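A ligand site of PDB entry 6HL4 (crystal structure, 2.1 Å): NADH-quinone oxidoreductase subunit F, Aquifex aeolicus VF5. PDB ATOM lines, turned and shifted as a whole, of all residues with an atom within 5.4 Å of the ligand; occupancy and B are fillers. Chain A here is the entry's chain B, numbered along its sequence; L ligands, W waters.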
ATOM      1  N   GLY A  65     -23.202  32.126  -8.612  1.00  0.00           N
ATOM      2  CA  GLY A  65     -23.514  31.793  -7.232  1.00  0.00           C
ATOM      3  C   GLY A  65     -22.453  32.250  -6.259  1.00  0.00           C
ATOM      4  O   GLY A  65     -21.256  32.186  -6.568  1.00  0.00           O
ATOM      5  N   ARG A  66     -22.889  32.782  -5.113  1.00  0.00           N
ATOM      6  CA  ARG A  66     -21.994  33.305  -4.070  1.00  0.00           C
ATOM      7  C   ARG A  66     -21.763  32.311  -2.909  1.00  0.00           C
ATOM      8  O   ARG A  66     -21.045  32.617  -1.960  1.00  0.00           O
ATOM      9  CB  ARG A  66     -22.490  34.687  -3.566  1.00  0.00           C
ATOM     10  CG  ARG A  66     -22.667  35.772  -4.640  1.00  0.00           C
ATOM     11  CD  ARG A  66     -21.391  36.131  -5.398  1.00  0.00           C
ATOM     12  NE  ARG A  66     -21.457  37.442  -6.015  1.00  0.00           N
ATOM     13  CZ  ARG A  66     -21.345  37.682  -7.315  1.00  0.00           C
ATOM     14  NH1 ARG A  66     -21.438  38.931  -7.780  1.00  0.00           N
ATOM     15  NH2 ARG A  66     -21.158  36.689  -8.170  1.00  0.00           N
ATOM     16  N   GLY A  67     -22.348  31.122  -3.056  1.00  0.00           N
ATOM     17  CA  GLY A  67     -22.294  30.057  -2.067  1.00  0.00           C
ATOM     18  C   GLY A  67     -21.153  29.069  -2.184  1.00  0.00           C
ATOM     19  O   GLY A  67     -21.234  27.980  -1.631  1.00  0.00           O
ATOM     20  N   GLY A  68     -20.111  29.449  -2.900  1.00  0.00           N
ATOM     21  CA  GLY A  68     -18.892  28.667  -3.051  1.00  0.00           C
ATOM     22  C   GLY A  68     -18.681  28.052  -4.410  1.00  0.00           C
ATOM     23  O   GLY A  68     -17.581  28.141  -4.968  1.00  0.00           O
ATOM     24  N   ALA A  69     -19.737  27.402  -4.945  1.00  0.00           N
ATOM     25  CA  ALA A  69     -19.728  26.665  -6.202  1.00  0.00           C
ATOM     26  C   ALA A  69     -19.628  27.529  -7.472  1.00  0.00           C
ATOM     27  O   ALA A  69     -19.277  27.018  -8.534  1.00  0.00           O
ATOM     28  CB  ALA A  69     -20.937  25.751  -6.278  1.00  0.00           C
ATOM     29  N   GLY A  70     -19.957  28.817  -7.342  1.00  0.00           N
ATOM     30  CA  GLY A  70     -19.907  29.800  -8.427  1.00  0.00           C
ATOM     31  C   GLY A  70     -20.640  29.440  -9.708  1.00  0.00           C
ATOM     32  O   GLY A  70     -20.156  29.750 -10.799  1.00  0.00           O
ATOM     33  N   PHE A  71     -21.809  28.776  -9.596  1.00  0.00           N
ATOM     34  CA  PHE A  71     -22.588  28.366 -10.766  1.00  0.00           C
ATOM     35  C   PHE A  71     -23.355  29.555 -11.362  1.00  0.00           C
ATOM     36  O   PHE A  71     -23.940  30.301 -10.585  1.00  0.00           O
ATOM     37  CB  PHE A  71     -23.543  27.213 -10.418  1.00  0.00           C
ATOM     38  CG  PHE A  71     -24.170  26.552 -11.629  1.00  0.00           C
ATOM     39  CD1 PHE A  71     -25.433  26.914 -12.067  1.00  0.00           C
ATOM     40  CD2 PHE A  71     -23.482  25.577 -12.338  1.00  0.00           C
ATOM     41  CE1 PHE A  71     -26.000  26.333 -13.200  1.00  0.00           C
ATOM     42  CE2 PHE A  71     -24.058  24.974 -13.464  1.00  0.00           C
ATOM     43  CZ  PHE A  71     -25.311  25.360 -13.887  1.00  0.00           C
ATOM     44  N   THR A  73     -26.090  31.829 -12.168  1.00  0.00           N
ATOM     45  CA  THR A  73     -27.453  31.903 -11.625  1.00  0.00           C
ATOM     46  C   THR A  73     -28.542  31.800 -12.701  1.00  0.00           C
ATOM     47  O   THR A  73     -29.487  31.042 -12.515  1.00  0.00           O
ATOM     48  CB  THR A  73     -27.594  33.142 -10.753  1.00  0.00           C
ATOM     49  OG1 THR A  73     -26.429  33.246  -9.939  1.00  0.00           O
ATOM     50  CG2 THR A  73     -28.838  33.106  -9.877  1.00  0.00           C
ATOM     51  N   LYS A  76     -28.873  28.185 -13.973  1.00  0.00           N
ATOM     52  CA  LYS A  76     -29.530  27.343 -12.971  1.00  0.00           C
ATOM     53  C   LYS A  76     -31.072  27.477 -13.068  1.00  0.00           C
ATOM     54  O   LYS A  76     -31.776  26.454 -13.049  1.00  0.00           O
ATOM     55  CB  LYS A  76     -29.045  27.719 -11.556  1.00  0.00           C
ATOM     56  CG  LYS A  76     -29.751  26.991 -10.423  1.00  0.00           C
ATOM     57  CD  LYS A  76     -29.391  27.552  -9.074  1.00  0.00           C
ATOM     58  CE  LYS A  76     -28.412  26.671  -8.360  1.00  0.00           C
ATOM     59  NZ  LYS A  76     -27.630  27.433  -7.366  1.00  0.00           N
ATOM     60  N   ASN A  92     -30.603  30.227   0.695  1.00  0.00           N
ATOM     61  CA  ASN A  92     -29.677  29.556   1.580  1.00  0.00           C
ATOM     62  C   ASN A  92     -28.989  30.523   2.554  1.00  0.00           C
ATOM     63  O   ASN A  92     -27.981  31.126   2.223  1.00  0.00           O
ATOM     64  CB  ASN A  92     -28.672  28.744   0.764  1.00  0.00           C
ATOM     65  CG  ASN A  92     -27.862  27.778   1.582  1.00  0.00           C
ATOM     66  OD1 ASN A  92     -27.737  27.903   2.805  1.00  0.00           O
ATOM     67  ND2 ASN A  92     -27.313  26.778   0.901  1.00  0.00           N
ATOM     68  N   ASP A  94     -27.696  29.482   5.441  1.00  0.00           N
ATOM     69  CA  ASP A  94     -27.081  28.561   6.383  1.00  0.00           C
ATOM     70  C   ASP A  94     -25.690  28.991   6.822  1.00  0.00           C
ATOM     71  O   ASP A  94     -25.292  28.607   7.938  1.00  0.00           O
ATOM     72  CB  ASP A  94     -27.068  27.127   5.872  1.00  0.00           C
ATOM     73  CG  ASP A  94     -26.849  26.138   7.005  1.00  0.00           C
ATOM     74  OD1 ASP A  94     -27.765  25.988   7.848  1.00  0.00           O
ATOM     75  OD2 ASP A  94     -25.756  25.556   7.070  1.00  0.00           O
ATOM     76  N   GLU A  95     -24.942  29.720   5.958  1.00  0.00           N
ATOM     77  CA  GLU A  95     -23.593  30.267   6.194  1.00  0.00           C
ATOM     78  C   GLU A  95     -22.935  29.787   7.507  1.00  0.00           C
ATOM     79  O   GLU A  95     -23.145  30.377   8.584  1.00  0.00           O
ATOM     80  CB  GLU A  95     -23.626  31.785   6.099  1.00  0.00           C
ATOM     81  CG  GLU A  95     -22.342  32.457   6.501  1.00  0.00           C
ATOM     82  CD  GLU A  95     -22.440  33.945   6.314  1.00  0.00           C
ATOM     83  OE1 GLU A  95     -22.901  34.646   7.241  1.00  0.00           O
ATOM     84  OE2 GLU A  95     -22.099  34.398   5.194  1.00  0.00           O
ATOM     85  N   SER A  96     -22.197  28.693   7.406  1.00  0.00           N
ATOM     86  CA  SER A  96     -21.593  28.078   8.578  1.00  0.00           C
ATOM     87  C   SER A  96     -20.103  27.765   8.394  1.00  0.00           C
ATOM     88  O   SER A  96     -19.484  27.242   9.322  1.00  0.00           O
ATOM     89  CB  SER A  96     -22.375  26.818   8.968  1.00  0.00           C
ATOM     90  OG  SER A  96     -23.597  27.134   9.622  1.00  0.00           O
ATOM     91  N   GLU A  97     -19.545  28.080   7.205  1.00  0.00           N
ATOM     92  CA  GLU A  97     -18.116  27.859   6.930  1.00  0.00           C
ATOM     93  C   GLU A  97     -17.282  28.814   7.802  1.00  0.00           C
ATOM     94  O   GLU A  97     -17.652  29.982   7.937  1.00  0.00           O
ATOM     95  CB  GLU A  97     -17.789  28.072   5.448  1.00  0.00           C
ATOM     96  CG  GLU A  97     -16.615  27.233   4.985  1.00  0.00           C
ATOM     97  CD  GLU A  97     -16.047  27.544   3.615  1.00  0.00           C
ATOM     98  OE1 GLU A  97     -16.839  27.817   2.682  1.00  0.00           O
ATOM     99  OE2 GLU A  97     -14.800  27.494   3.468  1.00  0.00           O
ATOM    100  N   ASP A 103     -23.225  37.031   4.822  1.00  0.00           N
ATOM    101  CA  ASP A 103     -24.667  36.886   4.586  1.00  0.00           C
ATOM    102  C   ASP A 103     -25.558  37.489   5.670  1.00  0.00           C
ATOM    103  O   ASP A 103     -26.557  38.115   5.329  1.00  0.00           O
ATOM    104  CB  ASP A 103     -25.038  35.411   4.326  1.00  0.00           C
ATOM    105  CG  ASP A 103     -24.390  34.837   3.065  1.00  0.00           C
ATOM    106  OD1 ASP A 103     -23.873  35.628   2.243  1.00  0.00           O
ATOM    107  OD2 ASP A 103     -24.373  33.580   2.923  1.00  0.00           O
ATOM    108  N   TYR A 180     -23.423  22.227   9.921  1.00  0.00           N
ATOM    109  CA  TYR A 180     -22.804  22.894   8.764  1.00  0.00           C
ATOM    110  C   TYR A 180     -23.281  22.255   7.474  1.00  0.00           C
ATOM    111  O   TYR A 180     -23.581  22.969   6.527  1.00  0.00           O
ATOM    112  CB  TYR A 180     -21.286  22.784   8.851  1.00  0.00           C
ATOM    113  CG  TYR A 180     -20.554  23.135   7.571  1.00  0.00           C
ATOM    114  CD1 TYR A 180     -20.559  24.438   7.077  1.00  0.00           C
ATOM    115  CD2 TYR A 180     -19.796  22.186   6.891  1.00  0.00           C
ATOM    116  CE1 TYR A 180     -19.879  24.768   5.906  1.00  0.00           C
ATOM    117  CE2 TYR A 180     -19.078  22.514   5.735  1.00  0.00           C
ATOM    118  CZ  TYR A 180     -19.129  23.819   5.244  1.00  0.00           C
ATOM    119  OH  TYR A 180     -18.452  24.183   4.115  1.00  0.00           O
ATOM    120  N   ILE A 181     -23.396  20.902   7.462  1.00  0.00           N
ATOM    121  CA  ILE A 181     -23.834  20.111   6.321  1.00  0.00           C
ATOM    122  C   ILE A 181     -25.201  20.583   5.751  1.00  0.00           C
ATOM    123  O   ILE A 181     -25.419  20.432   4.554  1.00  0.00           O
ATOM    124  CB  ILE A 181     -23.803  18.591   6.632  1.00  0.00           C
ATOM    125  CG1 ILE A 181     -23.798  17.719   5.352  1.00  0.00           C
ATOM    126  CG2 ILE A 181     -24.917  18.140   7.611  1.00  0.00           C
ATOM    127  CD1 ILE A 181     -22.634  17.962   4.451  1.00  0.00           C
ATOM    128  N   GLY A 183     -26.004  23.316   4.896  1.00  0.00           N
ATOM    129  CA  GLY A 183     -25.681  24.352   3.925  1.00  0.00           C
ATOM    130  C   GLY A 183     -25.582  23.763   2.530  1.00  0.00           C
ATOM    131  O   GLY A 183     -25.728  24.482   1.528  1.00  0.00           O
ATOM    132  N   GLU A 184     -25.324  22.436   2.457  1.00  0.00           N
ATOM    133  CA  GLU A 184     -25.276  21.649   1.238  1.00  0.00           C
ATOM    134  C   GLU A 184     -26.746  21.608   0.750  1.00  0.00           C
ATOM    135  O   GLU A 184     -27.657  21.312   1.553  1.00  0.00           O
ATOM    136  CB  GLU A 184     -24.707  20.245   1.579  1.00  0.00           C
ATOM    137  CG  GLU A 184     -24.169  19.464   0.404  1.00  0.00           C
ATOM    138  CD  GLU A 184     -25.189  18.722  -0.430  1.00  0.00           C
ATOM    139  OE1 GLU A 184     -26.321  18.457   0.062  1.00  0.00           O
ATOM    140  OE2 GLU A 184     -24.852  18.394  -1.587  1.00  0.00           O
ATOM    141  N   GLU A 185     -27.002  22.026  -0.512  1.00  0.00           N
ATOM    142  CA  GLU A 185     -28.346  22.207  -1.080  1.00  0.00           C
ATOM    143  C   GLU A 185     -29.324  21.002  -0.914  1.00  0.00           C
ATOM    144  O   GLU A 185     -30.495  21.245  -0.606  1.00  0.00           O
ATOM    145  CB  GLU A 185     -28.309  22.683  -2.545  1.00  0.00           C
ATOM    146  CG  GLU A 185     -27.678  21.721  -3.549  1.00  0.00           C
ATOM    147  CD  GLU A 185     -27.632  22.211  -4.989  1.00  0.00           C
ATOM    148  OE1 GLU A 185     -28.620  22.827  -5.455  1.00  0.00           O
ATOM    149  OE2 GLU A 185     -26.604  21.949  -5.660  1.00  0.00           O
ATOM    150  N   VAL A 218     -32.031  26.551  -5.313  1.00  0.00           N
ATOM    151  CA  VAL A 218     -31.379  26.943  -4.067  1.00  0.00           C
ATOM    152  C   VAL A 218     -30.329  27.958  -4.460  1.00  0.00           C
ATOM    153  O   VAL A 218     -29.449  27.674  -5.269  1.00  0.00           O
ATOM    154  CB  VAL A 218     -30.769  25.774  -3.266  1.00  0.00           C
ATOM    155  CG1 VAL A 218     -30.103  26.275  -1.982  1.00  0.00           C
ATOM    156  CG2 VAL A 218     -31.830  24.710  -2.952  1.00  0.00           C
ATOM    157  N   ASN A 219     -30.470  29.167  -3.914  1.00  0.00           N
ATOM    158  CA  ASN A 219     -29.539  30.243  -4.163  1.00  0.00           C
ATOM    159  C   ASN A 219     -29.108  30.825  -2.838  1.00  0.00           C
ATOM    160  O   ASN A 219     -29.871  30.807  -1.878  1.00  0.00           O
ATOM    161  CB  ASN A 219     -30.148  31.311  -5.071  1.00  0.00           C
ATOM    162  CG  ASN A 219     -29.844  31.112  -6.536  1.00  0.00           C
ATOM    163  OD1 ASN A 219     -30.733  31.110  -7.376  1.00  0.00           O
ATOM    164  ND2 ASN A 219     -28.565  30.938  -6.874  1.00  0.00           N
ATOM    165  N   ASN A 220     -27.855  31.276  -2.771  1.00  0.00           N
ATOM    166  CA  ASN A 220     -27.276  31.863  -1.590  1.00  0.00           C
ATOM    167  C   ASN A 220     -27.829  33.271  -1.360  1.00  0.00           C
ATOM    168  O   ASN A 220     -28.202  33.949  -2.327  1.00  0.00           O
ATOM    169  CB  ASN A 220     -25.741  31.871  -1.714  1.00  0.00           C
ATOM    170  CG  ASN A 220     -25.015  32.650  -0.647  1.00  0.00           C
ATOM    171  OD1 ASN A 220     -24.601  33.772  -0.875  1.00  0.00           O
ATOM    172  ND2 ASN A 220     -24.862  32.092   0.541  1.00  0.00           N
ATOM    173  N   VAL A 221     -27.889  33.704  -0.077  1.00  0.00           N
ATOM    174  CA  VAL A 221     -28.334  35.048   0.351  1.00  0.00           C
ATOM    175  C   VAL A 221     -27.731  36.137  -0.525  1.00  0.00           C
ATOM    176  O   VAL A 221     -28.456  36.981  -1.056  1.00  0.00           O
ATOM    177  CB  VAL A 221     -27.981  35.302   1.831  1.00  0.00           C
ATOM    178  CG1 VAL A 221     -28.219  36.775   2.225  1.00  0.00           C
ATOM    179  CG2 VAL A 221     -28.761  34.397   2.738  1.00  0.00           C
ATOM    180  N   THR A 223     -26.117  35.941  -3.479  1.00  0.00           N
ATOM    181  CA  THR A 223     -26.524  35.805  -4.896  1.00  0.00           C
ATOM    182  C   THR A 223     -27.896  36.490  -5.144  1.00  0.00           C
ATOM    183  O   THR A 223     -28.032  37.245  -6.110  1.00  0.00           O
ATOM    184  CB  THR A 223     -26.600  34.322  -5.303  1.00  0.00           C
ATOM    185  OG1 THR A 223     -25.565  33.609  -4.654  1.00  0.00           O
ATOM    186  CG2 THR A 223     -26.518  34.130  -6.796  1.00  0.00           C
ATOM    187  N   CYS A 393     -21.235  14.100  -1.245  1.00  0.00           N
ATOM    188  CA  CYS A 393     -21.352  15.558  -1.158  1.00  0.00           C
ATOM    189  C   CYS A 393     -19.974  16.235  -1.117  1.00  0.00           C
ATOM    190  O   CYS A 393     -18.963  15.564  -0.966  1.00  0.00           O
ATOM    191  CB  CYS A 393     -22.250  16.003   0.000  1.00  0.00           C
ATOM    192  SG  CYS A 393     -21.351  16.516   1.491  1.00  0.00           S
ATOM    193  N   GLY A 394     -19.962  17.551  -1.288  1.00  0.00           N
ATOM    194  CA  GLY A 394     -18.759  18.369  -1.355  1.00  0.00           C
ATOM    195  C   GLY A 394     -17.841  18.390  -0.145  1.00  0.00           C
ATOM    196  O   GLY A 394     -16.652  18.675  -0.309  1.00  0.00           O
ATOM    197  N   LEU A 395     -18.360  18.095   1.073  1.00  0.00           N
ATOM    198  CA  LEU A 395     -17.565  18.106   2.318  1.00  0.00           C
ATOM    199  C   LEU A 395     -16.417  17.103   2.248  1.00  0.00           C
ATOM    200  O   LEU A 395     -15.265  17.472   2.522  1.00  0.00           O
ATOM    201  CB  LEU A 395     -18.446  17.856   3.556  1.00  0.00           C
ATOM    202  CG  LEU A 395     -17.809  18.134   4.928  1.00  0.00           C
ATOM    203  CD1 LEU A 395     -18.822  18.625   5.939  1.00  0.00           C
ATOM    204  CD2 LEU A 395     -17.114  16.917   5.472  1.00  0.00           C
HETATM  205  N1  LIG L   1     -24.071  27.524   0.131  1.00  0.00           N
HETATM  206  C1  LIG L   1     -24.615  28.558   0.835  1.00  0.00           C
HETATM  207  O1  LIG L   1     -25.340  29.391   0.282  1.00  0.00           O
HETATM  208  N2  LIG L   1     -24.477  28.609   2.227  1.00  0.00           N
HETATM  209  C2  LIG L   1     -23.867  27.654   3.015  1.00  0.00           C
HETATM  210  O2  LIG L   1     -23.872  27.765   4.237  1.00  0.00           O
HETATM  211  C3  LIG L   1     -23.316  26.535   2.260  1.00  0.00           C
HETATM  212  N3  LIG L   1     -22.789  25.542   2.926  1.00  0.00           N
HETATM  213  C4  LIG L   1     -22.376  24.421   2.212  1.00  0.00           C
HETATM  214  C5  LIG L   1     -21.878  23.324   2.921  1.00  0.00           C
HETATM  215  C6  LIG L   1     -21.442  22.183   2.271  1.00  0.00           C
HETATM  216  C7  LIG L   1     -20.927  21.017   3.086  1.00  0.00           C
HETATM  217  C8  LIG L   1     -21.489  22.126   0.852  1.00  0.00           C
HETATM  218  C9  LIG L   1     -20.892  20.974   0.085  1.00  0.00           C
HETATM  219  C10 LIG L   1     -22.021  23.207   0.150  1.00  0.00           C
HETATM  220  C11 LIG L   1     -22.478  24.344   0.802  1.00  0.00           C
HETATM  221  N4  LIG L   1     -23.061  25.437   0.111  1.00  0.00           N
HETATM  222  C12 LIG L   1     -23.480  26.555   0.813  1.00  0.00           C
HETATM  223  C13 LIG L   1     -23.266  25.356  -1.341  1.00  0.00           C
HETATM  224  C14 LIG L   1     -24.650  24.861  -1.734  1.00  0.00           C
HETATM  225  O3  LIG L   1     -24.629  23.431  -1.872  1.00  0.00           O
HETATM  226  C15 LIG L   1     -25.133  25.477  -3.039  1.00  0.00           C
HETATM  227  O4  LIG L   1     -24.128  25.333  -4.036  1.00  0.00           O
HETATM  228  C16 LIG L   1     -25.567  26.951  -2.999  1.00  0.00           C
HETATM  229  O5  LIG L   1     -26.482  27.210  -1.933  1.00  0.00           O
HETATM  230  C17 LIG L   1     -26.179  27.378  -4.313  1.00  0.00           C
HETATM  231  O6  LIG L   1     -26.455  28.790  -4.271  1.00  0.00           O
HETATM  232  P1  LIG L   1     -25.614  29.796  -5.219  1.00  0.00           P
HETATM  233  O7  LIG L   1     -24.213  29.883  -4.750  1.00  0.00           O
HETATM  234  O8  LIG L   1     -25.731  29.314  -6.663  1.00  0.00           O
HETATM  235  O9  LIG L   1     -26.363  31.104  -5.103  1.00  0.00           O
HETATM  236  O   HOH W   1     -22.733  21.858  -3.260  1.00  0.00           O
HETATM  237  O   HOH W   2     -25.550  31.189   3.397  1.00  0.00           O
HETATM  238  O   HOH W   3     -23.345  28.179  -7.317  1.00  0.00           O
HETATM  239  O   HOH W   4     -26.192  30.381  -9.114  1.00  0.00           O
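The side-chain hydroxyl of Thr 223 is in hydrogen-bond range of an oxygen (O9) of the ligand, 2.7 Å away. The backbone NH (N) of Asn 220 sits at hydrogen-bond distance from an oxygen (O9) of the ligand, at 2.8 Å. The side-chain amide nitrogen (ND2) of Asn 220 is in hydrogen-bond range of an oxygen (O1) of the ligand (2.8 Å). NZ of Lys 76 lies within salt-bridge range of O8 of the ligand, 2.8 Å away. The backbone NH of Gly 67 is in hydrogen-bond range of an oxygen (O7) of the ligand, at 2.8 Å. The backbone NH (N) of Glu 95 lies within hydrogen-bond range of an oxygen (O2) of the ligand. An oxygen (O9) of the ligand is in hydrogen-bond range of the side-chain amide nitrogen (ND2) of Asn 219 (2.8 Å). ND2 of Asn 92 is in hydrogen-bond range of O5 of the ligand (3.0 Å). An oxygen (O3) of the ligand lies within hydrogen-bond range of the backbone NH (N) of Glu 185, 3.1 Å away. An oxygen (O7) of the ligand is in hydrogen-bond range of the backbone NH (N) of Arg 66 (3.2 Å).
The side-chain hydroxyl (OG1) of Thr 223 lies within hydrogen-bond range of the backbone NH (N) of Arg 66, at 2.8 Å. The side-chain amide nitrogen (ND2) of Asn 220 sits at hydrogen-bond distance from the side-chain carboxylate (OD2) of Asp 103, at 2.9 Å. OE2 of Glu 95 sits at hydrogen-bond distance from N of Asp 103, at 2.9 Å. O of Asn 219 sits at hydrogen-bond distance from N of Asn 92. The side-chain amide nitrogen (ND2) of Asn 92 sits at hydrogen-bond distance from the backbone carbonyl oxygen (O) of Gly 183 (2.9 Å). N of Val 221 sits close to O of Asn 92. OD2 of Asp 94 sits at hydrogen-bond distance from N of Gly 183 (3.1 Å). SG of Cys 393 sits close to N of Leu 395.
N4 of the ligand lies close to O of Gly 183 (3.2 Å). O6 of the ligand sits close to O of Val 218, 3.3 Å away. Residues that only touch the ligand: Gly 65 (3.2 Å), Asp 94 (3.4 Å), Tyr 180 (3.6 Å), Glu 184 (3.6 Å), Gly 394 (3.7 Å), Ser 96 (3.7 Å), Ile 181 (3.8 Å), Ala 69 (3.9 Å) and Leu 395 (3.96 Å). 20 residues have an atom within 4 Å of the ligand: Gly 65, Arg 66, Gly 67, Ala 69, Lys 76, Asn 92, Asp 94, Glu 95, Ser 96, Tyr 180, Ile 181, Gly 183, Glu 184, Glu 185, Val 218, Asn 219, Asn 220, Thr 223, Gly 394 and Leu 395.
Water W4 lies within hydrogen-bond range of the backbone carbonyl oxygen (O) of Phe 71 (2.7 Å), an oxygen (O8) of the ligand (2.7 Å), the side-chain hydroxyl (OG1) of Thr 73 (3.0 Å), the side-chain amide nitrogen (ND2) of Asn 219 (3.3 Å) and the backbone NH (N) of Gly 65 (3.5 Å). Water W3 lies within hydrogen-bond range of an oxygen (O8) of the ligand (2.7 Å), the backbone NH of Phe 71 (2.8 Å) and the backbone NH of Gly 70 (3.4 Å).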
